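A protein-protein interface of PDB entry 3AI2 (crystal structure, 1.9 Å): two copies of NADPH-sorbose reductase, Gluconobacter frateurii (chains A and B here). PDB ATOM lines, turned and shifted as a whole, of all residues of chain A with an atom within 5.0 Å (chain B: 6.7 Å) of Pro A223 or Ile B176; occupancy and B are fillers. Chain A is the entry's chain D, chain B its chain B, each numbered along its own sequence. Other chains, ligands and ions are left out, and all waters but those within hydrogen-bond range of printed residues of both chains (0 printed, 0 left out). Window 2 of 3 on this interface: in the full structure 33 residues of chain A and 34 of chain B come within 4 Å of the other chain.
The backbone NH (N) of Gly A258 is in hydrogen-bond range of the backbone carbonyl oxygen (O) of Val B249 (3.2 Å).
The backbone NH (N) of Ile A224 lies within hydrogen-bond range of the backbone carbonyl oxygen (O) of Gly A257 (3.1 Å).
Among the printed residues, merely in contact across the chains: Gly A257 with Val B249, Pro A223 with Ile B176, Ile A224 with Ile B176 and Ile A224 with Thr B246.
Of chain B, only Ile B176 (3.6 Å) comes within 4 Å of Pro A223. Of the printed residues of chain B, Ile A224 touches Ile B176 and Thr B246. Printed residues of chain A within 4 Å of Thr B246: Ile A224. Of the printed residues of chain B, Gly A258 touches Val B249. Printed residues of chain B within 4 Å of Gly A257: Val B249. Of the printed residues of chain A, Val B249 touches Gly A257 (3.6 Å) and Gly A258 (3.2 Å). Lys B177 touches none of the printed residues of chain A. The nearest residue of chain B that does not touch Pro A223 is Thr B173 (4.9 Å). The nearest printed residue of chain B that does not touch Gly A258 is Ser B248 (5.6 Å).
Printed residues of chain A that touch a printed residue of chain B: Pro A223, Ile A224, Gly A257 and Gly A258. Hydrophobic or aromatic side chains of chain B within 4 Å of the printed part of chain A: Ile B176 and Val B249. Among the printed residues, 5 pairs touch across the chains.
No position is printed for both chains.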
ATOM      1  N   HIS A 221     -25.344  33.407  18.304  1.00  0.00           N
ATOM      2  CA  HIS A 221     -26.174  32.215  18.473  1.00  0.00           C
ATOM      3  C   HIS A 221     -25.538  31.154  19.328  1.00  0.00           C
ATOM      4  O   HIS A 221     -26.234  30.415  19.966  1.00  0.00           O
ATOM      5  CB  HIS A 221     -26.546  31.613  17.104  1.00  0.00           C
ATOM      6  CG  HIS A 221     -27.645  32.349  16.403  1.00  0.00           C
ATOM      7  ND1 HIS A 221     -27.484  32.939  15.164  1.00  0.00           N
ATOM      8  CD2 HIS A 221     -28.914  32.625  16.788  1.00  0.00           C
ATOM      9  CE1 HIS A 221     -28.619  33.520  14.803  1.00  0.00           C
ATOM     10  NE2 HIS A 221     -29.499  33.352  15.775  1.00  0.00           N
ATOM     11  N   ALA A 222     -24.215  31.054  19.353  1.00  0.00           N
ATOM     12  CA  ALA A 222     -23.584  29.869  19.944  1.00  0.00           C
ATOM     13  C   ALA A 222     -22.562  30.261  21.011  1.00  0.00           C
ATOM     14  O   ALA A 222     -21.603  30.986  20.703  1.00  0.00           O
ATOM     15  CB  ALA A 222     -22.900  29.039  18.847  1.00  0.00           C
ATOM     16  N   PRO A 223     -22.721  29.736  22.228  1.00  0.00           N
ATOM     17  CA  PRO A 223     -21.766  29.879  23.333  1.00  0.00           C
ATOM     18  C   PRO A 223     -20.327  29.502  22.953  1.00  0.00           C
ATOM     19  O   PRO A 223     -19.380  30.137  23.424  1.00  0.00           O
ATOM     20  CB  PRO A 223     -22.301  28.895  24.371  1.00  0.00           C
ATOM     21  CG  PRO A 223     -23.811  28.927  24.118  1.00  0.00           C
ATOM     22  CD  PRO A 223     -23.947  29.019  22.641  1.00  0.00           C
ATOM     23  N   ILE A 224     -20.150  28.488  22.115  1.00  0.00           N
ATOM     24  CA  ILE A 224     -18.789  28.115  21.707  1.00  0.00           C
ATOM     25  C   ILE A 224     -18.196  29.151  20.679  1.00  0.00           C
ATOM     26  O   ILE A 224     -17.023  29.076  20.306  1.00  0.00           O
ATOM     27  CB  ILE A 224     -18.789  26.725  21.085  1.00  0.00           C
ATOM     28  CG1 ILE A 224     -17.388  26.092  21.084  1.00  0.00           C
ATOM     29  CG2 ILE A 224     -19.454  26.755  19.648  1.00  0.00           C
ATOM     30  CD1 ILE A 224     -17.475  24.671  20.609  1.00  0.00           C
ATOM     31  N   LYS A 225     -19.042  30.032  20.177  1.00  0.00           N
ATOM     32  CA  LYS A 225     -18.564  31.173  19.380  1.00  0.00           C
ATOM     33  C   LYS A 225     -17.774  30.769  18.108  1.00  0.00           C
ATOM     34  O   LYS A 225     -16.850  31.472  17.679  1.00  0.00           O
ATOM     35  CB  LYS A 225     -17.808  32.142  20.299  1.00  0.00           C
ATOM     36  CG  LYS A 225     -18.808  32.793  21.243  1.00  0.00           C
ATOM     37  CD  LYS A 225     -18.456  34.186  21.673  1.00  0.00           C
ATOM     38  CE  LYS A 225     -17.784  34.166  23.013  1.00  0.00           C
ATOM     39  NZ  LYS A 225     -16.487  33.467  22.785  1.00  0.00           N
ATOM     40  N   GLY A 257     -23.179  23.286  19.702  1.00  0.00           N
ATOM     41  CA  GLY A 257     -22.209  24.232  20.323  1.00  0.00           C
ATOM     42  C   GLY A 257     -22.801  25.127  21.395  1.00  0.00           C
ATOM     43  O   GLY A 257     -22.334  26.286  21.609  1.00  0.00           O
ATOM     44  N   GLY A 258     -23.876  24.637  22.023  1.00  0.00           N
ATOM     45  CA  GLY A 258     -24.575  25.454  23.033  1.00  0.00           C
ATOM     46  C   GLY A 258     -25.765  26.259  22.535  1.00  0.00           C
ATOM     47  O   GLY A 258     -26.422  26.949  23.337  1.00  0.00           O
ATOM     48  N   MET A 259     -26.070  26.199  21.220  1.00  0.00           N
ATOM     49  CA  MET A 259     -27.046  27.109  20.661  1.00  0.00           C
ATOM     50  C   MET A 259     -28.441  26.892  21.215  1.00  0.00           C
ATOM     51  O   MET A 259     -29.221  27.827  21.232  1.00  0.00           O
ATOM     52  CB  MET A 259     -27.093  26.957  19.133  1.00  0.00           C
ATOM     53  CG  MET A 259     -27.984  28.012  18.403  1.00  0.00           C
ATOM     54  SD  MET A 259     -27.766  27.752  16.599  1.00  0.00           S
ATOM     55  CE  MET A 259     -29.194  28.665  15.972  1.00  0.00           C
ATOM     56  N   LEU B 171     -23.726  24.931  33.909  1.00  0.00           N
ATOM     57  CA  LEU B 171     -22.256  24.737  33.869  1.00  0.00           C
ATOM     58  C   LEU B 171     -21.691  24.824  32.452  1.00  0.00           C
ATOM     59  O   LEU B 171     -20.689  25.544  32.204  1.00  0.00           O
ATOM     60  CB  LEU B 171     -21.830  23.419  34.565  1.00  0.00           C
ATOM     61  CG  LEU B 171     -20.310  23.296  34.756  1.00  0.00           C
ATOM     62  CD1 LEU B 171     -19.822  24.342  35.815  1.00  0.00           C
ATOM     63  CD2 LEU B 171     -19.933  21.822  35.160  1.00  0.00           C
ATOM     64  N   ALA B 172     -22.379  24.203  31.488  1.00  0.00           N
ATOM     65  CA  ALA B 172     -21.870  24.176  30.134  1.00  0.00           C
ATOM     66  C   ALA B 172     -21.660  25.611  29.614  1.00  0.00           C
ATOM     67  O   ALA B 172     -20.687  25.899  28.920  1.00  0.00           O
ATOM     68  CB  ALA B 172     -22.851  23.441  29.185  1.00  0.00           C
ATOM     69  N   THR B 173     -22.595  26.498  29.912  1.00  0.00           N
ATOM     70  CA  THR B 173     -22.486  27.896  29.393  1.00  0.00           C
ATOM     71  C   THR B 173     -21.431  28.649  30.145  1.00  0.00           C
ATOM     72  O   THR B 173     -20.754  29.501  29.576  1.00  0.00           O
ATOM     73  CB  THR B 173     -23.842  28.676  29.447  1.00  0.00           C
ATOM     74  OG1 THR B 173     -24.243  28.821  30.813  1.00  0.00           O
ATOM     75  CG2 THR B 173     -24.892  27.853  28.773  1.00  0.00           C
ATOM     76  N   GLU B 174     -21.274  28.349  31.422  1.00  0.00           N
ATOM     77  CA  GLU B 174     -20.203  28.983  32.158  1.00  0.00           C
ATOM     78  C   GLU B 174     -18.760  28.577  31.738  1.00  0.00           C
ATOM     79  O   GLU B 174     -17.867  29.426  31.748  1.00  0.00           O
ATOM     80  CB  GLU B 174     -20.354  28.710  33.651  1.00  0.00           C
ATOM     81  CG  GLU B 174     -19.452  29.592  34.493  1.00  0.00           C
ATOM     82  CD  GLU B 174     -19.728  29.477  35.989  1.00  0.00           C
ATOM     83  OE1 GLU B 174     -20.928  29.603  36.408  1.00  0.00           O
ATOM     84  OE2 GLU B 174     -18.733  29.292  36.740  1.00  0.00           O
ATOM     85  N   VAL B 175     -18.502  27.288  31.469  1.00  0.00           N
ATOM     86  CA  VAL B 175     -17.086  26.870  31.264  1.00  0.00           C
ATOM     87  C   VAL B 175     -16.692  26.625  29.826  1.00  0.00           C
ATOM     88  O   VAL B 175     -15.528  26.278  29.552  1.00  0.00           O
ATOM     89  CB  VAL B 175     -16.777  25.638  32.079  1.00  0.00           C
ATOM     90  CG1 VAL B 175     -17.092  25.951  33.529  1.00  0.00           C
ATOM     91  CG2 VAL B 175     -17.656  24.449  31.602  1.00  0.00           C
ATOM     92  N   ILE B 176     -17.624  26.792  28.880  1.00  0.00           N
ATOM     93  CA  ILE B 176     -17.217  26.632  27.486  1.00  0.00           C
ATOM     94  C   ILE B 176     -16.059  27.630  27.135  1.00  0.00           C
ATOM     95  O   ILE B 176     -15.225  27.316  26.295  1.00  0.00           O
ATOM     96  CB  ILE B 176     -18.416  26.691  26.450  1.00  0.00           C
ATOM     97  CG1 ILE B 176     -17.939  26.366  25.033  1.00  0.00           C
ATOM     98  CG2 ILE B 176     -19.049  28.070  26.404  1.00  0.00           C
ATOM     99  CD1 ILE B 176     -17.368  24.979  24.861  1.00  0.00           C
ATOM    100  N   LYS B 177     -15.980  28.758  27.838  1.00  0.00           N
ATOM    101  CA  LYS B 177     -14.941  29.780  27.538  1.00  0.00           C
ATOM    102  C   LYS B 177     -13.565  29.198  27.892  1.00  0.00           C
ATOM    103  O   LYS B 177     -12.536  29.713  27.469  1.00  0.00           O
ATOM    104  CB  LYS B 177     -15.191  31.059  28.358  1.00  0.00           C
ATOM    105  CG  LYS B 177     -15.158  30.848  29.894  1.00  0.00           C
ATOM    106  CD  LYS B 177     -15.410  32.164  30.737  1.00  0.00           C
ATOM    107  CE  LYS B 177     -16.851  32.698  30.671  1.00  0.00           C
ATOM    108  NZ  LYS B 177     -17.827  32.183  31.747  1.00  0.00           N
ATOM    109  N   ASP B 178     -13.565  28.138  28.726  1.00  0.00           N
ATOM    110  CA  ASP B 178     -12.332  27.450  29.122  1.00  0.00           C
ATOM    111  C   ASP B 178     -12.031  26.272  28.231  1.00  0.00           C
ATOM    112  O   ASP B 178     -11.192  25.438  28.583  1.00  0.00           O
ATOM    113  CB  ASP B 178     -12.453  26.924  30.553  1.00  0.00           C
ATOM    114  CG  ASP B 178     -12.635  28.025  31.579  1.00  0.00           C
ATOM    115  OD1 ASP B 178     -12.137  29.169  31.403  1.00  0.00           O
ATOM    116  OD2 ASP B 178     -13.295  27.723  32.594  1.00  0.00           O
ATOM    117  N   ASN B 179     -12.733  26.169  27.100  1.00  0.00           N
ATOM    118  CA  ASN B 179     -12.599  24.997  26.256  1.00  0.00           C
ATOM    119  C   ASN B 179     -12.972  23.727  27.039  1.00  0.00           C
ATOM    120  O   ASN B 179     -12.422  22.641  26.815  1.00  0.00           O
ATOM    121  CB  ASN B 179     -11.173  24.839  25.639  1.00  0.00           C
ATOM    122  CG  ASN B 179     -11.146  23.834  24.475  1.00  0.00           C
ATOM    123  OD1 ASN B 179     -12.059  23.815  23.659  1.00  0.00           O
ATOM    124  ND2 ASN B 179     -10.086  23.011  24.380  1.00  0.00           N
ATOM    125  N   ILE B 180     -13.904  23.869  27.985  1.00  0.00           N
ATOM    126  CA  ILE B 180     -14.510  22.692  28.630  1.00  0.00           C
ATOM    127  C   ILE B 180     -15.962  22.464  28.127  1.00  0.00           C
ATOM    128  O   ILE B 180     -16.810  23.358  28.243  1.00  0.00           O
ATOM    129  CB  ILE B 180     -14.527  22.922  30.151  1.00  0.00           C
ATOM    130  CG1 ILE B 180     -13.070  22.952  30.616  1.00  0.00           C
ATOM    131  CG2 ILE B 180     -15.242  21.726  30.895  1.00  0.00           C
ATOM    132  CD1 ILE B 180     -12.920  23.455  32.051  1.00  0.00           C
ATOM    133  N   ARG B 181     -16.215  21.271  27.619  1.00  0.00           N
ATOM    134  CA  ARG B 181     -17.522  20.886  27.076  1.00  0.00           C
ATOM    135  C   ARG B 181     -18.267  20.050  28.110  1.00  0.00           C
ATOM    136  O   ARG B 181     -17.799  18.972  28.497  1.00  0.00           O
ATOM    137  CB  ARG B 181     -17.357  20.067  25.790  1.00  0.00           C
ATOM    138  CG  ARG B 181     -16.701  20.812  24.656  1.00  0.00           C
ATOM    139  CD  ARG B 181     -16.597  19.873  23.405  1.00  0.00           C
ATOM    140  NE  ARG B 181     -15.881  18.580  23.576  1.00  0.00           N
ATOM    141  CZ  ARG B 181     -16.465  17.395  23.893  1.00  0.00           C
ATOM    142  NH1 ARG B 181     -17.790  17.328  24.152  1.00  0.00           N
ATOM    143  NH2 ARG B 181     -15.734  16.258  23.985  1.00  0.00           N
ATOM    144  N   VAL B 182     -19.432  20.549  28.531  1.00  0.00           N
ATOM    145  CA  VAL B 182     -20.249  19.885  29.561  1.00  0.00           C
ATOM    146  C   VAL B 182     -21.556  19.415  28.905  1.00  0.00           C
ATOM    147  O   VAL B 182     -22.203  20.158  28.166  1.00  0.00           O
ATOM    148  CB  VAL B 182     -20.580  20.865  30.729  1.00  0.00           C
ATOM    149  CG1 VAL B 182     -21.466  20.191  31.780  1.00  0.00           C
ATOM    150  CG2 VAL B 182     -19.257  21.499  31.284  1.00  0.00           C
ATOM    151  N   THR B 246     -16.606  17.302  19.579  1.00  0.00           N
ATOM    152  CA  THR B 246     -16.137  18.617  19.955  1.00  0.00           C
ATOM    153  C   THR B 246     -17.170  19.710  19.743  1.00  0.00           C
ATOM    154  O   THR B 246     -16.903  20.893  20.083  1.00  0.00           O
ATOM    155  CB  THR B 246     -14.838  18.953  19.147  1.00  0.00           C
ATOM    156  OG1 THR B 246     -15.053  18.610  17.772  1.00  0.00           O
ATOM    157  CG2 THR B 246     -13.665  18.128  19.706  1.00  0.00           C
ATOM    158  N   SER B 248     -20.427  19.193  20.836  1.00  0.00           N
ATOM    159  CA  SER B 248     -21.472  18.938  21.829  1.00  0.00           C
ATOM    160  C   SER B 248     -21.255  19.798  23.061  1.00  0.00           C
ATOM    161  O   SER B 248     -20.265  19.644  23.747  1.00  0.00           O
ATOM    162  CB  SER B 248     -21.529  17.440  22.178  1.00  0.00           C
ATOM    163  OG  SER B 248     -21.862  16.711  21.027  1.00  0.00           O
ATOM    164  N   VAL B 249     -22.189  20.719  23.316  1.00  0.00           N
ATOM    165  CA  VAL B 249     -22.104  21.655  24.402  1.00  0.00           C
ATOM    166  C   VAL B 249     -23.496  21.920  24.991  1.00  0.00           C
ATOM    167  O   VAL B 249     -24.409  22.385  24.293  1.00  0.00           O
ATOM    168  CB  VAL B 249     -21.507  23.021  23.973  1.00  0.00           C
ATOM    169  CG1 VAL B 249     -21.434  24.021  25.159  1.00  0.00           C
ATOM    170  CG2 VAL B 249     -20.093  22.845  23.290  1.00  0.00           C
